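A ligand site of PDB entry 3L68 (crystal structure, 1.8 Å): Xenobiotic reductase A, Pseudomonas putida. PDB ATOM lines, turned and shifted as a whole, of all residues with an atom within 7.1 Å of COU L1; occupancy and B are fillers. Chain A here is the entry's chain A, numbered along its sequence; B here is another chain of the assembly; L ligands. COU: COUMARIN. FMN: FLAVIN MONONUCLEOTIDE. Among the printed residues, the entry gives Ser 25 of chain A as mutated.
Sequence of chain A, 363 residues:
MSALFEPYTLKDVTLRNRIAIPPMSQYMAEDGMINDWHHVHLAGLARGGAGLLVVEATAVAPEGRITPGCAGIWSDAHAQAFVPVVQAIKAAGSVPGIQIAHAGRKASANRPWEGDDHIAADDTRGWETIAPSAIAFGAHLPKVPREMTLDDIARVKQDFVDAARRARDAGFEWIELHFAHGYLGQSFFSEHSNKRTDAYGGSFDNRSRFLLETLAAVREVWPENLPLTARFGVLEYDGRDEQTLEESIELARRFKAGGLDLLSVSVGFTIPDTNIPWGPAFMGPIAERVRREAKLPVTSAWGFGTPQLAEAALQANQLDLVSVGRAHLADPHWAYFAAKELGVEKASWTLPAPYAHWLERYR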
ATOM      1  N   PRO A  23      20.412 -19.962  21.624  1.00  0.00           N
ATOM      2  CA  PRO A  23      19.359 -19.528  22.551  1.00  0.00           C
ATOM      3  C   PRO A  23      19.470 -20.308  23.848  1.00  0.00           C
ATOM      4  O   PRO A  23      19.623 -21.557  23.818  1.00  0.00           O
ATOM      5  CB  PRO A  23      18.063 -19.895  21.820  1.00  0.00           C
ATOM      6  CG  PRO A  23      18.481 -20.926  20.783  1.00  0.00           C
ATOM      7  CD  PRO A  23      19.856 -20.504  20.372  1.00  0.00           C
ATOM      8  N   MET A  24      19.438 -19.594  24.960  1.00  0.00           N
ATOM      9  CA  MET A  24      19.408 -20.187  26.285  1.00  0.00           C
ATOM     10  C   MET A  24      18.376 -19.470  27.178  1.00  0.00           C
ATOM     11  O   MET A  24      18.630 -18.386  27.704  1.00  0.00           O
ATOM     12  CB  MET A  24      20.793 -20.173  26.928  1.00  0.00           C
ATOM     13  CG  MET A  24      21.722 -21.267  26.408  1.00  0.00           C
ATOM     14  SD  MET A  24      23.344 -21.180  27.186  1.00  0.00           S
ATOM     15  CE  MET A  24      23.909 -19.575  26.626  1.00  0.00           C
ATOM     16  N   SER A  25      17.227 -20.111  27.334  1.00  0.00           N
ATOM     17  CA  SER A  25      16.158 -19.627  28.206  1.00  0.00           C
ATOM     18  C   SER A  25      16.687 -19.281  29.607  1.00  0.00           C
ATOM     19  O   SER A  25      17.501 -20.010  30.175  1.00  0.00           O
ATOM     20  CB  SER A  25      15.060 -20.684  28.311  1.00  0.00           C
ATOM     21  OG  SER A  25      14.423 -20.900  27.061  1.00  0.00           O
ATOM     22  N   TYR A  27      14.364 -17.893  32.042  1.00  0.00           N
ATOM     23  CA  TYR A  27      13.203 -18.042  32.918  1.00  0.00           C
ATOM     24  C   TYR A  27      13.054 -16.867  33.894  1.00  0.00           C
ATOM     25  O   TYR A  27      12.574 -17.047  35.025  1.00  0.00           O
ATOM     26  CB  TYR A  27      13.269 -19.384  33.665  1.00  0.00           C
ATOM     27  CG  TYR A  27      13.534 -20.566  32.775  1.00  0.00           C
ATOM     28  CD1 TYR A  27      12.496 -21.221  32.113  1.00  0.00           C
ATOM     29  CD2 TYR A  27      14.832 -21.038  32.593  1.00  0.00           C
ATOM     30  CE1 TYR A  27      12.752 -22.309  31.287  1.00  0.00           C
ATOM     31  CE2 TYR A  27      15.088 -22.138  31.773  1.00  0.00           C
ATOM     32  CZ  TYR A  27      14.043 -22.758  31.121  1.00  0.00           C
ATOM     33  OH  TYR A  27      14.296 -23.847  30.309  1.00  0.00           O
ATOM     34  N   ALA A  57      14.562 -18.763  23.475  1.00  0.00           N
ATOM     35  CA  ALA A  57      13.228 -19.025  22.948  1.00  0.00           C
ATOM     36  C   ALA A  57      12.247 -17.958  23.420  1.00  0.00           C
ATOM     37  O   ALA A  57      12.075 -17.749  24.613  1.00  0.00           O
ATOM     38  CB  ALA A  57      12.742 -20.410  23.384  1.00  0.00           C
ATOM     39  N   ILE A  66       7.211 -21.929  27.522  1.00  0.00           N
ATOM     40  CA  ILE A  66       7.428 -23.184  28.217  1.00  0.00           C
ATOM     41  C   ILE A  66       6.949 -23.018  29.654  1.00  0.00           C
ATOM     42  O   ILE A  66       6.283 -23.914  30.197  1.00  0.00           O
ATOM     43  CB  ILE A  66       8.912 -23.600  28.225  1.00  0.00           C
ATOM     44  CG1 ILE A  66       9.498 -23.605  26.814  1.00  0.00           C
ATOM     45  CG2 ILE A  66       9.066 -24.962  28.870  1.00  0.00           C
ATOM     46  CD1 ILE A  66      10.997 -23.841  26.784  1.00  0.00           C
ATOM     47  N   GLN A  99      15.495 -16.365  18.755  1.00  0.00           N
ATOM     48  CA  GLN A  99      14.730 -17.565  18.445  1.00  0.00           C
ATOM     49  C   GLN A  99      13.253 -17.363  18.822  1.00  0.00           C
ATOM     50  O   GLN A  99      12.946 -17.067  19.970  1.00  0.00           O
ATOM     51  CB  GLN A  99      15.284 -18.767  19.204  1.00  0.00           C
ATOM     52  CG  GLN A  99      14.549 -20.062  18.905  1.00  0.00           C
ATOM     53  CD  GLN A  99      14.966 -21.189  19.820  1.00  0.00           C
ATOM     54  OE1 GLN A  99      14.724 -21.131  21.037  1.00  0.00           O
ATOM     55  NE2 GLN A  99      15.594 -22.215  19.267  1.00  0.00           N
ATOM     56  N   PRO A 112      13.010 -24.914  35.542  1.00  0.00           N
ATOM     57  CA  PRO A 112      13.801 -26.121  35.809  1.00  0.00           C
ATOM     58  C   PRO A 112      14.232 -26.256  37.272  1.00  0.00           C
ATOM     59  O   PRO A 112      14.237 -27.382  37.790  1.00  0.00           O
ATOM     60  CB  PRO A 112      14.991 -25.963  34.867  1.00  0.00           C
ATOM     61  CG  PRO A 112      14.426 -25.152  33.709  1.00  0.00           C
ATOM     62  CD  PRO A 112      13.512 -24.157  34.381  1.00  0.00           C
ATOM     63  N   ASP A 116      10.662 -28.390  37.310  1.00  0.00           N
ATOM     64  CA  ASP A 116      10.885 -28.747  35.904  1.00  0.00           C
ATOM     65  C   ASP A 116       9.716 -29.513  35.273  1.00  0.00           C
ATOM     66  O   ASP A 116       9.822 -29.989  34.138  1.00  0.00           O
ATOM     67  CB  ASP A 116      12.193 -29.556  35.758  1.00  0.00           C
ATOM     68  CG  ASP A 116      12.733 -29.550  34.326  1.00  0.00           C
ATOM     69  OD1 ASP A 116      12.719 -28.472  33.679  1.00  0.00           O
ATOM     70  OD2 ASP A 116      13.203 -30.612  33.850  1.00  0.00           O
ATOM     71  N   HIS A 178      11.980 -21.965  15.976  1.00  0.00           N
ATOM     72  CA  HIS A 178      12.220 -23.097  16.888  1.00  0.00           C
ATOM     73  C   HIS A 178      11.385 -24.313  16.521  1.00  0.00           C
ATOM     74  O   HIS A 178      10.294 -24.519  17.080  1.00  0.00           O
ATOM     75  CB  HIS A 178      11.925 -22.710  18.335  1.00  0.00           C
ATOM     76  CG  HIS A 178      12.571 -23.622  19.339  1.00  0.00           C
ATOM     77  ND1 HIS A 178      13.168 -24.802  18.976  1.00  0.00           N
ATOM     78  CD2 HIS A 178      12.713 -23.516  20.686  1.00  0.00           C
ATOM     79  CE1 HIS A 178      13.661 -25.395  20.054  1.00  0.00           C
ATOM     80  NE2 HIS A 178      13.396 -24.634  21.101  1.00  0.00           N
ATOM     81  N   ALA A 180      12.395 -27.397  17.015  1.00  0.00           N
ATOM     82  CA  ALA A 180      13.136 -28.516  17.599  1.00  0.00           C
ATOM     83  C   ALA A 180      12.709 -28.830  19.030  1.00  0.00           C
ATOM     84  O   ALA A 180      11.789 -28.200  19.567  1.00  0.00           O
ATOM     85  CB  ALA A 180      14.633 -28.241  17.535  1.00  0.00           C
ATOM     86  N   HIS A 181      13.376 -29.809  19.635  1.00  0.00           N
ATOM     87  CA  HIS A 181      13.282 -30.092  21.071  1.00  0.00           C
ATOM     88  C   HIS A 181      11.871 -30.459  21.566  1.00  0.00           C
ATOM     89  O   HIS A 181      11.540 -30.293  22.756  1.00  0.00           O
ATOM     90  CB  HIS A 181      13.886 -28.939  21.889  1.00  0.00           C
ATOM     91  CG  HIS A 181      15.323 -28.660  21.548  1.00  0.00           C
ATOM     92  ND1 HIS A 181      15.966 -27.490  21.928  1.00  0.00           N
ATOM     93  CD2 HIS A 181      16.233 -29.381  20.858  1.00  0.00           C
ATOM     94  CE1 HIS A 181      17.220 -27.522  21.491  1.00  0.00           C
ATOM     95  NE2 HIS A 181      17.407 -28.649  20.837  1.00  0.00           N
ATOM     96  N   TYR A 183       8.910 -29.317  20.974  1.00  0.00           N
ATOM     97  CA  TYR A 183       7.878 -28.286  21.088  1.00  0.00           C
ATOM     98  C   TYR A 183       6.954 -28.373  19.864  1.00  0.00           C
ATOM     99  O   TYR A 183       6.977 -29.371  19.156  1.00  0.00           O
ATOM    100  CB  TYR A 183       8.517 -26.899  21.249  1.00  0.00           C
ATOM    101  CG  TYR A 183       9.464 -26.848  22.445  1.00  0.00           C
ATOM    102  CD1 TYR A 183       9.007 -27.133  23.729  1.00  0.00           C
ATOM    103  CD2 TYR A 183      10.814 -26.542  22.286  1.00  0.00           C
ATOM    104  CE1 TYR A 183       9.855 -27.088  24.828  1.00  0.00           C
ATOM    105  CE2 TYR A 183      11.672 -26.500  23.394  1.00  0.00           C
ATOM    106  CZ  TYR A 183      11.183 -26.776  24.652  1.00  0.00           C
ATOM    107  OH  TYR A 183      12.022 -26.753  25.754  1.00  0.00           O
ATOM    108  N   ARG A 231      15.889 -24.032  13.918  1.00  0.00           N
ATOM    109  CA  ARG A 231      16.449 -25.130  14.681  1.00  0.00           C
ATOM    110  C   ARG A 231      15.527 -26.345  14.522  1.00  0.00           C
ATOM    111  O   ARG A 231      14.314 -26.217  14.600  1.00  0.00           O
ATOM    112  CB  ARG A 231      16.614 -24.755  16.158  1.00  0.00           C
ATOM    113  CG  ARG A 231      17.563 -25.713  16.916  1.00  0.00           C
ATOM    114  CD  ARG A 231      18.019 -25.161  18.280  1.00  0.00           C
ATOM    115  NE  ARG A 231      19.356 -25.679  18.613  1.00  0.00           N
ATOM    116  CZ  ARG A 231      20.027 -25.400  19.731  1.00  0.00           C
ATOM    117  NH1 ARG A 231      21.238 -25.926  19.918  1.00  0.00           N
ATOM    118  NH2 ARG A 231      19.507 -24.616  20.662  1.00  0.00           N
ATOM    119  N   PHE A 269      13.987 -34.623  20.946  1.00  0.00           N
ATOM    120  CA  PHE A 269      13.371 -34.668  22.275  1.00  0.00           C
ATOM    121  C   PHE A 269      11.834 -34.724  22.243  1.00  0.00           C
ATOM    122  O   PHE A 269      11.184 -34.209  23.141  1.00  0.00           O
ATOM    123  CB  PHE A 269      13.845 -33.495  23.166  1.00  0.00           C
ATOM    124  CG  PHE A 269      15.339 -33.416  23.315  1.00  0.00           C
ATOM    125  CD1 PHE A 269      16.014 -34.313  24.152  1.00  0.00           C
ATOM    126  CD2 PHE A 269      16.074 -32.478  22.622  1.00  0.00           C
ATOM    127  CE1 PHE A 269      17.389 -34.252  24.278  1.00  0.00           C
ATOM    128  CE2 PHE A 269      17.447 -32.406  22.756  1.00  0.00           C
ATOM    129  CZ  PHE A 269      18.111 -33.300  23.585  1.00  0.00           C
ATOM    130  N   TRP A 302      26.564 -28.809  21.872  1.00  0.00           N
ATOM    131  CA  TRP A 302      26.784 -29.824  22.914  1.00  0.00           C
ATOM    132  C   TRP A 302      28.250 -30.218  23.065  1.00  0.00           C
ATOM    133  O   TRP A 302      28.748 -31.116  22.372  1.00  0.00           O
ATOM    134  CB  TRP A 302      25.886 -31.066  22.807  1.00  0.00           C
ATOM    135  CG  TRP A 302      26.020 -31.897  24.060  1.00  0.00           C
ATOM    136  CD1 TRP A 302      27.026 -32.780  24.366  1.00  0.00           C
ATOM    137  CD2 TRP A 302      25.160 -31.872  25.208  1.00  0.00           C
ATOM    138  NE1 TRP A 302      26.826 -33.322  25.608  1.00  0.00           N
ATOM    139  CE2 TRP A 302      25.699 -32.782  26.150  1.00  0.00           C
ATOM    140  CE3 TRP A 302      23.991 -31.180  25.533  1.00  0.00           C
ATOM    141  CZ2 TRP A 302      25.087 -33.011  27.391  1.00  0.00           C
ATOM    142  CZ3 TRP A 302      23.395 -31.409  26.755  1.00  0.00           C
ATOM    143  CH2 TRP A 302      23.945 -32.323  27.670  1.00  0.00           C
ATOM    144  N   TRP B 358      22.536 -25.010  35.870  1.00  0.00           N
ATOM    145  CA  TRP B 358      23.018 -25.779  34.717  1.00  0.00           C
ATOM    146  C   TRP B 358      24.480 -26.153  34.812  1.00  0.00           C
ATOM    147  O   TRP B 358      24.981 -26.932  34.007  1.00  0.00           O
ATOM    148  CB  TRP B 358      22.787 -24.991  33.422  1.00  0.00           C
ATOM    149  CG  TRP B 358      21.408 -24.478  33.340  1.00  0.00           C
ATOM    150  CD1 TRP B 358      20.988 -23.204  33.599  1.00  0.00           C
ATOM    151  CD2 TRP B 358      20.235 -25.236  33.034  1.00  0.00           C
ATOM    152  NE1 TRP B 358      19.623 -23.117  33.452  1.00  0.00           N
ATOM    153  CE2 TRP B 358      19.138 -24.355  33.109  1.00  0.00           C
ATOM    154  CE3 TRP B 358      20.008 -26.572  32.699  1.00  0.00           C
ATOM    155  CZ2 TRP B 358      17.832 -24.764  32.840  1.00  0.00           C
ATOM    156  CZ3 TRP B 358      18.712 -26.985  32.439  1.00  0.00           C
ATOM    157  CH2 TRP B 358      17.642 -26.091  32.519  1.00  0.00           C
HETATM  158  C1  COU L   1      15.054 -25.507  24.804  1.00  0.00           C
HETATM  159  C2  COU L   1      14.503 -24.627  25.724  1.00  0.00           C
HETATM  160  C3  COU L   1      14.955 -24.642  27.043  1.00  0.00           C
HETATM  161  C4  COU L   1      15.943 -25.552  27.408  1.00  0.00           C
HETATM  162  C5  COU L   1      16.418 -25.587  28.715  1.00  0.00           C
HETATM  163  C6  COU L   1      17.412 -26.492  29.074  1.00  0.00           C
HETATM  164  C7  COU L   1      17.941 -27.365  28.136  1.00  0.00           C
HETATM  165  C8  COU L   1      17.472 -27.325  26.824  1.00  0.00           C
HETATM  166  C9  COU L   1      16.478 -26.420  26.464  1.00  0.00           C
HETATM  167  O1  COU L   1      14.657 -25.512  23.616  1.00  0.00           O
HETATM  168  O2  COU L   1      16.025 -26.404  25.182  1.00  0.00           O
HETATM  169  N1  FMN L   2      17.826 -24.416  23.130  1.00  0.00           N
HETATM  170  C2  FMN L   2      16.823 -23.829  22.394  1.00  0.00           C
HETATM  171  O2  FMN L   2      16.615 -24.207  21.241  1.00  0.00           O
HETATM  172  N3  FMN L   2      16.042 -22.828  22.931  1.00  0.00           N
HETATM  173  C4  FMN L   2      16.274 -22.401  24.230  1.00  0.00           C
HETATM  174  O4  FMN L   2      15.592 -21.488  24.719  1.00  0.00           O
HETATM  175  C4A FMN L   2      17.288 -22.991  24.975  1.00  0.00           C
HETATM  176  N5  FMN L   2      17.512 -22.572  26.257  1.00  0.00           N
HETATM  177  C5A FMN L   2      18.525 -23.149  26.997  1.00  0.00           C
HETATM  178  C6  FMN L   2      18.744 -22.708  28.294  1.00  0.00           C
HETATM  179  C7  FMN L   2      19.755 -23.271  29.063  1.00  0.00           C
HETATM  180  C7M FMN L   2      19.960 -22.751  30.459  1.00  0.00           C
HETATM  181  C8  FMN L   2      20.548 -24.287  28.541  1.00  0.00           C
HETATM  182  C8M FMN L   2      21.641 -24.890  29.378  1.00  0.00           C
HETATM  183  C9  FMN L   2      20.326 -24.733  27.235  1.00  0.00           C
HETATM  184  C9A FMN L   2      19.304 -24.167  26.457  1.00  0.00           C
HETATM  185  N10 FMN L   2      19.066 -24.600  25.164  1.00  0.00           N
HETATM  186  C10 FMN L   2      18.068 -23.995  24.416  1.00  0.00           C
HETATM  187  C1' FMN L   2      19.924 -25.673  24.533  1.00  0.00           C
HETATM  188  C2' FMN L   2      21.203 -24.925  24.142  1.00  0.00           C
HETATM  189  O2' FMN L   2      20.878 -23.965  23.163  1.00  0.00           O
HETATM  190  C3' FMN L   2      22.336 -25.846  23.660  1.00  0.00           C
HETATM  191  O3' FMN L   2      21.927 -26.638  22.556  1.00  0.00           O
HETATM  192  C4' FMN L   2      22.810 -26.790  24.782  1.00  0.00           C
HETATM  193  O4' FMN L   2      23.112 -26.066  25.969  1.00  0.00           O
HETATM  194  C5' FMN L   2      24.043 -27.594  24.364  1.00  0.00           C
HETATM  195  O5' FMN L   2      25.166 -26.759  24.156  1.00  0.00           O
HETATM  196  P   FMN L   2      26.311 -26.617  25.302  1.00  0.00           P
HETATM  197  O1P FMN L   2      25.657 -26.010  26.518  1.00  0.00           O
HETATM  198  O2P FMN L   2      26.876 -27.949  25.698  1.00  0.00           O
HETATM  199  O3P FMN L   2      27.413 -25.729  24.785  1.00  0.00           O
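A ring nitrogen (ND1) of His 181 sits at hydrogen-bond distance from an oxygen (O1) of COU L1 (2.9 Å). NE2 of His 178 is in hydrogen-bond range of O1 of COU L1 (2.9 Å). O2 of FMN L2 lies close to ND1 of His 181 (3.4 Å). A ring nitrogen (NE2) of His 178 sits at hydrogen-bond distance from an oxygen (O2) of FMN L2 (3.3 Å). N of Ser 25 lies within hydrogen-bond range of N5 of FMN L2 (2.7 Å). An oxygen (O4) of FMN L2 is in hydrogen-bond range of the side-chain hydroxyl of Ser 25, at 2.7 Å. N3 of FMN L2 lies within hydrogen-bond range of OE1 of Gln 99 (2.9 Å). The backbone NH (N) of Ala 57 lies within hydrogen-bond range of an oxygen (O4) of FMN L2 (3.2 Å). NH1 of Arg 231 is in hydrogen-bond range of O3' of FMN L2 (2.8 Å). O of Pro 23 sits at hydrogen-bond distance from O2' of FMN L2. The backbone NH of Trp 302 lies within hydrogen-bond range of an oxygen (O5') of FMN L2 (3.4 Å).
An oxygen (O1) of COU L1 sits close to a nitrogen (N3) of FMN L2 (3.1 Å).
The backbone NH (N) of Ala 180 lies close to a ring nitrogen (ND1) of His 178.
Ser 25 touches COU L1 (OG to C3, 3.8 Å). OH of Tyr 27 touches C5 of COU L1, at 3.2 Å. CD1 of Ile 66 touches C2 of COU L1, 3.7 Å away. Tyr 183 touches COU L1. Trp 358 of chain B touches COU L1 (CH2 to C6, 3.5 Å). Hydrophobic or aromatic side chains that line COU L1: Ile 66, His 178, His 181, Tyr 183 and Trp 358 of chain B. Within 4 Å of COU L1: Ser 25, Tyr 27, Ile 66, His 178, His 181, Tyr 183 and Trp 358 of chain B.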
